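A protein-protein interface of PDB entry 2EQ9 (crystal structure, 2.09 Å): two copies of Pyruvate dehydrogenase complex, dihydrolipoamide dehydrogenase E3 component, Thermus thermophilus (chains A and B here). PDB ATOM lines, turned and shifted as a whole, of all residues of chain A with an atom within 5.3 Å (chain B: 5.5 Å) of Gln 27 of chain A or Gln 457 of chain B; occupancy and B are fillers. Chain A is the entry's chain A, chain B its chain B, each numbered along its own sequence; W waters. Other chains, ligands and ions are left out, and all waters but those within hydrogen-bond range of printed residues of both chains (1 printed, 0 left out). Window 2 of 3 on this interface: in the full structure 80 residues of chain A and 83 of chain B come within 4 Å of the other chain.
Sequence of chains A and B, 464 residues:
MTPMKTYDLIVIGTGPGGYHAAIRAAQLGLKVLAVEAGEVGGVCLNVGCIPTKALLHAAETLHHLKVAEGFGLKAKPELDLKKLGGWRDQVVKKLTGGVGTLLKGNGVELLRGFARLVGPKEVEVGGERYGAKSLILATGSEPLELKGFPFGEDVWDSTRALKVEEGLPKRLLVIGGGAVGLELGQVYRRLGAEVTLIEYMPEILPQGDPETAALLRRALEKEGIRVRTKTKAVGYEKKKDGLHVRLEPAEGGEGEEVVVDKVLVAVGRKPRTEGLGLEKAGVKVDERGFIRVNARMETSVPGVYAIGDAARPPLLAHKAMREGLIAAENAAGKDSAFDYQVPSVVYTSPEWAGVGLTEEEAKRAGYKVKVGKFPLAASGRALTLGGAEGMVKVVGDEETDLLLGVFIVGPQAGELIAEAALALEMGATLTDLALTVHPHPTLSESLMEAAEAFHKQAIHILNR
The side-chain carboxylate (OE1) of Glu 452 of chain B is in salt-bridge range of the guanidinium group (NH2) of Arg 24 of chain A. The guanidinium group of Arg 24 of chain A lies within hydrogen-bond range of the backbone carbonyl oxygen of Gln 457 of chain B, 3.0 Å away. The side-chain amide nitrogen (NE2) of Gln 27 of chain A lies within hydrogen-bond range of the backbone carbonyl oxygen (O) of Gln 457 of chain B (3.5 Å). O of Ala 458 of chain B is in hydrogen-bond range of NE2 of Gln 27 of chain A (2.8 Å). The side-chain amide nitrogen of Gln 27 of chain A sits close to the side-chain amide nitrogen of Asn 463 of chain B, 3.3 Å away.
The guanidinium group of Arg 24 of chain A sits at hydrogen-bond distance from the side-chain amide oxygen of Gln 27 of chain A, at 2.8 Å. The guanidinium group (NH1) of Arg 24 of chain A lies within salt-bridge range of the side-chain carboxylate (OE1) of Glu 329 of chain A (2.8 Å). N of Gln 457 of chain B is in hydrogen-bond range of O of Glu 452 of chain B, at 3.0 Å. The backbone carbonyl oxygen of Ala 458 of chain B is in hydrogen-bond range of the side-chain amide nitrogen of Asn 463 of chain B.
CG2 of Ile 23 of chain A touches CD1 of Ile 459 of chain B, at 3.8 Å. Arg 24 of chain A touches Ile 459 of chain B (N to CD1, 3.998 Å).
Of the printed residues of chain B, Arg 24 of chain A touches Glu 452 (3.2 Å), Gln 457 (3.0 Å) and Ile 459 (3.998 Å). Of the printed residues of chain B, Gln 27 of chain A touches Gln 457, Ala 458 and Asn 463. Leu 28 of chain A touches none of the printed residues of chain B. Of the printed residues of chain A, Glu 452 of chain B touches Arg 24. Of the printed residues of chain A, Gln 457 of chain B touches Arg 24 and Gln 27. Printed residues of chain A within 4 Å of Ala 458 of chain B: Gln 27 (2.8 Å). Of the printed residues of chain A, Ile 459 of chain B touches Ile 23 and Arg 24. The nearest residue of chain A that does not touch Gln 457 of chain B is Glu 329 of chain A (5.0 Å).
Of the 10 printed residues of chain A, 3 touch a printed residue of chain B. Printed residues of chain A that touch a printed residue of chain B: Ile 23, Arg 24 and Gln 27. Hydrophobic or aromatic side chains of chain A within 4 Å of the printed part of chain B: Ile 23. Along chain A the printed residues that touch a printed residue of chain B span positions 23 to 27. Of the 9 printed residues of chain B, 5 touch a printed residue of chain A. Printed residues of chain B that touch a printed residue of chain A: Glu 452, Gln 457, Ala 458, Ile 459 and Asn 463. Hydrophobic or aromatic side chains of chain B that line the printed part of chain A: Ile 459.
No position is printed for both chains. Of the 7 pairs that touch across the chains among the printed residues, none has its exchanged pair printed and touching as well.
Water W1 lies within hydrogen-bond range of the backbone carbonyl oxygen of Ile 459 of chain B (2.8 Å), the backbone carbonyl oxygen of Ile 461 of chain B (2.9 Å) and the side-chain amide nitrogen of Asn 106 of chain A (3.0 Å).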
ATOM      1  N   ALA A  22      25.988 -16.697   7.241  1.00  0.00           N
ATOM      2  CA  ALA A  22      24.591 -16.476   7.602  1.00  0.00           C
ATOM      3  C   ALA A  22      23.955 -17.734   8.183  1.00  0.00           C
ATOM      4  O   ALA A  22      23.339 -17.696   9.248  1.00  0.00           O
ATOM      5  CB  ALA A  22      23.801 -16.010   6.386  1.00  0.00           C
ATOM      6  N   ILE A  23      24.113 -18.852   7.483  1.00  0.00           N
ATOM      7  CA  ILE A  23      23.536 -20.106   7.932  1.00  0.00           C
ATOM      8  C   ILE A  23      24.170 -20.638   9.218  1.00  0.00           C
ATOM      9  O   ILE A  23      23.452 -21.001  10.157  1.00  0.00           O
ATOM     10  CB  ILE A  23      23.606 -21.166   6.819  1.00  0.00           C
ATOM     11  CG1 ILE A  23      22.724 -20.719   5.645  1.00  0.00           C
ATOM     12  CG2 ILE A  23      23.137 -22.517   7.348  1.00  0.00           C
ATOM     13  CD1 ILE A  23      22.674 -21.693   4.485  1.00  0.00           C
ATOM     14  N   ARG A  24      25.499 -20.686   9.285  1.00  0.00           N
ATOM     15  CA  ARG A  24      26.138 -21.174  10.506  1.00  0.00           C
ATOM     16  C   ARG A  24      25.715 -20.293  11.686  1.00  0.00           C
ATOM     17  O   ARG A  24      25.467 -20.791  12.775  1.00  0.00           O
ATOM     18  CB  ARG A  24      27.666 -21.171  10.361  1.00  0.00           C
ATOM     19  CG  ARG A  24      28.445 -21.583  11.623  1.00  0.00           C
ATOM     20  CD  ARG A  24      27.950 -22.886  12.233  1.00  0.00           C
ATOM     21  NE  ARG A  24      27.959 -24.019  11.308  1.00  0.00           N
ATOM     22  CZ  ARG A  24      29.032 -24.747  11.001  1.00  0.00           C
ATOM     23  NH1 ARG A  24      30.210 -24.465  11.550  1.00  0.00           N
ATOM     24  NH2 ARG A  24      28.926 -25.769  10.155  1.00  0.00           N
ATOM     25  N   ALA A  25      25.627 -18.986  11.460  1.00  0.00           N
ATOM     26  CA  ALA A  25      25.219 -18.071  12.518  1.00  0.00           C
ATOM     27  C   ALA A  25      23.790 -18.384  12.983  1.00  0.00           C
ATOM     28  O   ALA A  25      23.508 -18.357  14.184  1.00  0.00           O
ATOM     29  CB  ALA A  25      25.319 -16.633  12.039  1.00  0.00           C
ATOM     30  N   ALA A  26      22.895 -18.682  12.041  1.00  0.00           N
ATOM     31  CA  ALA A  26      21.519 -19.016  12.395  1.00  0.00           C
ATOM     32  C   ALA A  26      21.474 -20.317  13.200  1.00  0.00           C
ATOM     33  O   ALA A  26      20.700 -20.439  14.149  1.00  0.00           O
ATOM     34  CB  ALA A  26      20.663 -19.156  11.142  1.00  0.00           C
ATOM     35  N   GLN A  27      22.293 -21.292  12.815  1.00  0.00           N
ATOM     36  CA  GLN A  27      22.324 -22.569  13.529  1.00  0.00           C
ATOM     37  C   GLN A  27      22.745 -22.333  14.972  1.00  0.00           C
ATOM     38  O   GLN A  27      22.362 -23.085  15.862  1.00  0.00           O
ATOM     39  CB  GLN A  27      23.307 -23.549  12.871  1.00  0.00           C
ATOM     40  CG  GLN A  27      23.018 -23.856  11.407  1.00  0.00           C
ATOM     41  CD  GLN A  27      24.082 -24.745  10.767  1.00  0.00           C
ATOM     42  OE1 GLN A  27      25.237 -24.747  11.187  1.00  0.00           O
ATOM     43  NE2 GLN A  27      23.696 -25.490   9.737  1.00  0.00           N
ATOM     44  N   LEU A  28      23.533 -21.284  15.197  1.00  0.00           N
ATOM     45  CA  LEU A  28      24.005 -20.962  16.540  1.00  0.00           C
ATOM     46  C   LEU A  28      23.007 -20.099  17.302  1.00  0.00           C
ATOM     47  O   LEU A  28      23.331 -19.541  18.348  1.00  0.00           O
ATOM     48  CB  LEU A  28      25.362 -20.259  16.475  1.00  0.00           C
ATOM     49  CG  LEU A  28      26.484 -21.127  15.915  1.00  0.00           C
ATOM     50  CD1 LEU A  28      27.745 -20.294  15.764  1.00  0.00           C
ATOM     51  CD2 LEU A  28      26.724 -22.315  16.844  1.00  0.00           C
ATOM     52  N   GLY A  29      21.798 -19.985  16.759  1.00  0.00           N
ATOM     53  CA  GLY A  29      20.748 -19.220  17.413  1.00  0.00           C
ATOM     54  C   GLY A  29      20.706 -17.719  17.199  1.00  0.00           C
ATOM     55  O   GLY A  29      19.981 -17.022  17.904  1.00  0.00           O
ATOM     56  N   ASN A 106      16.466 -21.558   7.269  1.00  0.00           N
ATOM     57  CA  ASN A 106      17.257 -21.372   8.480  1.00  0.00           C
ATOM     58  C   ASN A 106      16.805 -20.149   9.268  1.00  0.00           C
ATOM     59  O   ASN A 106      17.375 -19.825  10.310  1.00  0.00           O
ATOM     60  CB  ASN A 106      18.739 -21.239   8.128  1.00  0.00           C
ATOM     61  CG  ASN A 106      19.421 -22.583   7.988  1.00  0.00           C
ATOM     62  OD1 ASN A 106      19.835 -23.184   8.981  1.00  0.00           O
ATOM     63  ND2 ASN A 106      19.526 -23.073   6.760  1.00  0.00           N
ATOM     64  N   GLU A 329      30.904 -18.199  13.790  1.00  0.00           N
ATOM     65  CA  GLU A 329      31.113 -18.763  15.109  1.00  0.00           C
ATOM     66  C   GLU A 329      31.631 -17.709  16.075  1.00  0.00           C
ATOM     67  O   GLU A 329      31.258 -17.707  17.252  1.00  0.00           O
ATOM     68  CB  GLU A 329      32.068 -19.957  15.023  1.00  0.00           C
ATOM     69  CG  GLU A 329      31.398 -21.171  14.392  1.00  0.00           C
ATOM     70  CD  GLU A 329      32.373 -22.260  13.998  1.00  0.00           C
ATOM     71  OE1 GLU A 329      31.910 -23.303  13.492  1.00  0.00           O
ATOM     72  OE2 GLU A 329      33.595 -22.077  14.186  1.00  0.00           O
ATOM     73  N   GLU B 452      29.582 -32.994   8.888  1.00  0.00           N
ATOM     74  CA  GLU B 452      28.938 -31.841   9.503  1.00  0.00           C
ATOM     75  C   GLU B 452      27.486 -32.164   9.881  1.00  0.00           C
ATOM     76  O   GLU B 452      26.981 -31.701  10.918  1.00  0.00           O
ATOM     77  CB  GLU B 452      28.974 -30.646   8.560  1.00  0.00           C
ATOM     78  CG  GLU B 452      30.379 -30.272   8.135  1.00  0.00           C
ATOM     79  CD  GLU B 452      30.468 -28.857   7.624  1.00  0.00           C
ATOM     80  OE1 GLU B 452      30.537 -27.926   8.461  1.00  0.00           O
ATOM     81  OE2 GLU B 452      30.457 -28.680   6.385  1.00  0.00           O
ATOM     82  N   ALA B 453      26.821 -32.959   9.044  1.00  0.00           N
ATOM     83  CA  ALA B 453      25.440 -33.336   9.317  1.00  0.00           C
ATOM     84  C   ALA B 453      25.411 -34.161  10.601  1.00  0.00           C
ATOM     85  O   ALA B 453      24.447 -34.121  11.356  1.00  0.00           O
ATOM     86  CB  ALA B 453      24.877 -34.141   8.158  1.00  0.00           C
ATOM     87  N   HIS B 455      26.992 -33.622  13.192  1.00  0.00           N
ATOM     88  CA  HIS B 455      26.936 -32.693  14.321  1.00  0.00           C
ATOM     89  C   HIS B 455      25.790 -31.695  14.158  1.00  0.00           C
ATOM     90  O   HIS B 455      25.761 -30.648  14.802  1.00  0.00           O
ATOM     91  CB  HIS B 455      28.264 -31.943  14.469  1.00  0.00           C
ATOM     92  CG  HIS B 455      29.401 -32.814  14.900  1.00  0.00           C
ATOM     93  ND1 HIS B 455      30.521 -33.017  14.123  1.00  0.00           N
ATOM     94  CD2 HIS B 455      29.583 -33.552  16.022  1.00  0.00           C
ATOM     95  CE1 HIS B 455      31.345 -33.842  14.746  1.00  0.00           C
ATOM     96  NE2 HIS B 455      30.799 -34.183  15.902  1.00  0.00           N
ATOM     97  N   LYS B 456      24.858 -32.031  13.277  1.00  0.00           N
ATOM     98  CA  LYS B 456      23.696 -31.202  13.023  1.00  0.00           C
ATOM     99  C   LYS B 456      24.003 -29.780  12.578  1.00  0.00           C
ATOM    100  O   LYS B 456      23.315 -28.835  12.971  1.00  0.00           O
ATOM    101  CB  LYS B 456      22.803 -31.188  14.269  1.00  0.00           C
ATOM    102  CG  LYS B 456      22.330 -32.580  14.658  1.00  0.00           C
ATOM    103  CD  LYS B 456      21.725 -33.280  13.444  1.00  0.00           C
ATOM    104  CE  LYS B 456      21.475 -34.762  13.685  1.00  0.00           C
ATOM    105  NZ  LYS B 456      21.209 -35.471  12.393  1.00  0.00           N
ATOM    106  N   GLN B 457      25.033 -29.621  11.758  1.00  0.00           N
ATOM    107  CA  GLN B 457      25.369 -28.295  11.256  1.00  0.00           C
ATOM    108  C   GLN B 457      25.777 -28.268   9.790  1.00  0.00           C
ATOM    109  O   GLN B 457      26.552 -27.408   9.368  1.00  0.00           O
ATOM    110  CB  GLN B 457      26.441 -27.629  12.127  1.00  0.00           C
ATOM    111  CG  GLN B 457      27.577 -28.519  12.568  1.00  0.00           C
ATOM    112  CD  GLN B 457      28.476 -27.809  13.567  1.00  0.00           C
ATOM    113  OE1 GLN B 457      28.002 -27.255  14.560  1.00  0.00           O
ATOM    114  NE2 GLN B 457      29.777 -27.822  13.308  1.00  0.00           N
ATOM    115  N   ALA B 458      25.257 -29.213   9.015  1.00  0.00           N
ATOM    116  CA  ALA B 458      25.538 -29.235   7.589  1.00  0.00           C
ATOM    117  C   ALA B 458      25.015 -27.892   7.087  1.00  0.00           C
ATOM    118  O   ALA B 458      24.088 -27.321   7.674  1.00  0.00           O
ATOM    119  CB  ALA B 458      24.790 -30.382   6.913  1.00  0.00           C
ATOM    120  N   ILE B 459      25.600 -27.382   6.011  1.00  0.00           N
ATOM    121  CA  ILE B 459      25.178 -26.093   5.481  1.00  0.00           C
ATOM    122  C   ILE B 459      24.270 -26.209   4.264  1.00  0.00           C
ATOM    123  O   ILE B 459      23.307 -25.451   4.136  1.00  0.00           O
ATOM    124  CB  ILE B 459      26.404 -25.224   5.100  1.00  0.00           C
ATOM    125  CG1 ILE B 459      27.270 -24.962   6.343  1.00  0.00           C
ATOM    126  CG2 ILE B 459      25.941 -23.901   4.476  1.00  0.00           C
ATOM    127  CD1 ILE B 459      26.660 -23.988   7.352  1.00  0.00           C
ATOM    128  N   ILE B 461      22.101 -28.509   3.424  1.00  0.00           N
ATOM    129  CA  ILE B 461      20.831 -29.190   3.633  1.00  0.00           C
ATOM    130  C   ILE B 461      20.361 -28.705   4.983  1.00  0.00           C
ATOM    131  O   ILE B 461      21.166 -28.272   5.802  1.00  0.00           O
ATOM    132  CB  ILE B 461      20.932 -30.728   3.710  1.00  0.00           C
ATOM    133  CG1 ILE B 461      21.960 -31.131   4.772  1.00  0.00           C
ATOM    134  CG2 ILE B 461      21.189 -31.297   2.333  1.00  0.00           C
ATOM    135  CD1 ILE B 461      22.017 -32.622   5.040  1.00  0.00           C
ATOM    136  N   ASN B 463      19.149 -29.170   8.630  1.00  0.00           N
ATOM    137  CA  ASN B 463      19.440 -30.193   9.624  1.00  0.00           C
ATOM    138  C   ASN B 463      18.265 -30.526  10.517  1.00  0.00           C
ATOM    139  O   ASN B 463      17.893 -31.720  10.556  1.00  0.00           O
ATOM    140  CB  ASN B 463      20.629 -29.748  10.463  1.00  0.00           C
ATOM    141  CG  ASN B 463      21.881 -29.581   9.628  1.00  0.00           C
ATOM    142  OD1 ASN B 463      22.575 -30.557   9.319  1.00  0.00           O
ATOM    143  ND2 ASN B 463      22.161 -28.343   9.233  1.00  0.00           N
HETATM  144  O   HOH W   1      21.270 -25.360   6.089  1.00  0.00           O
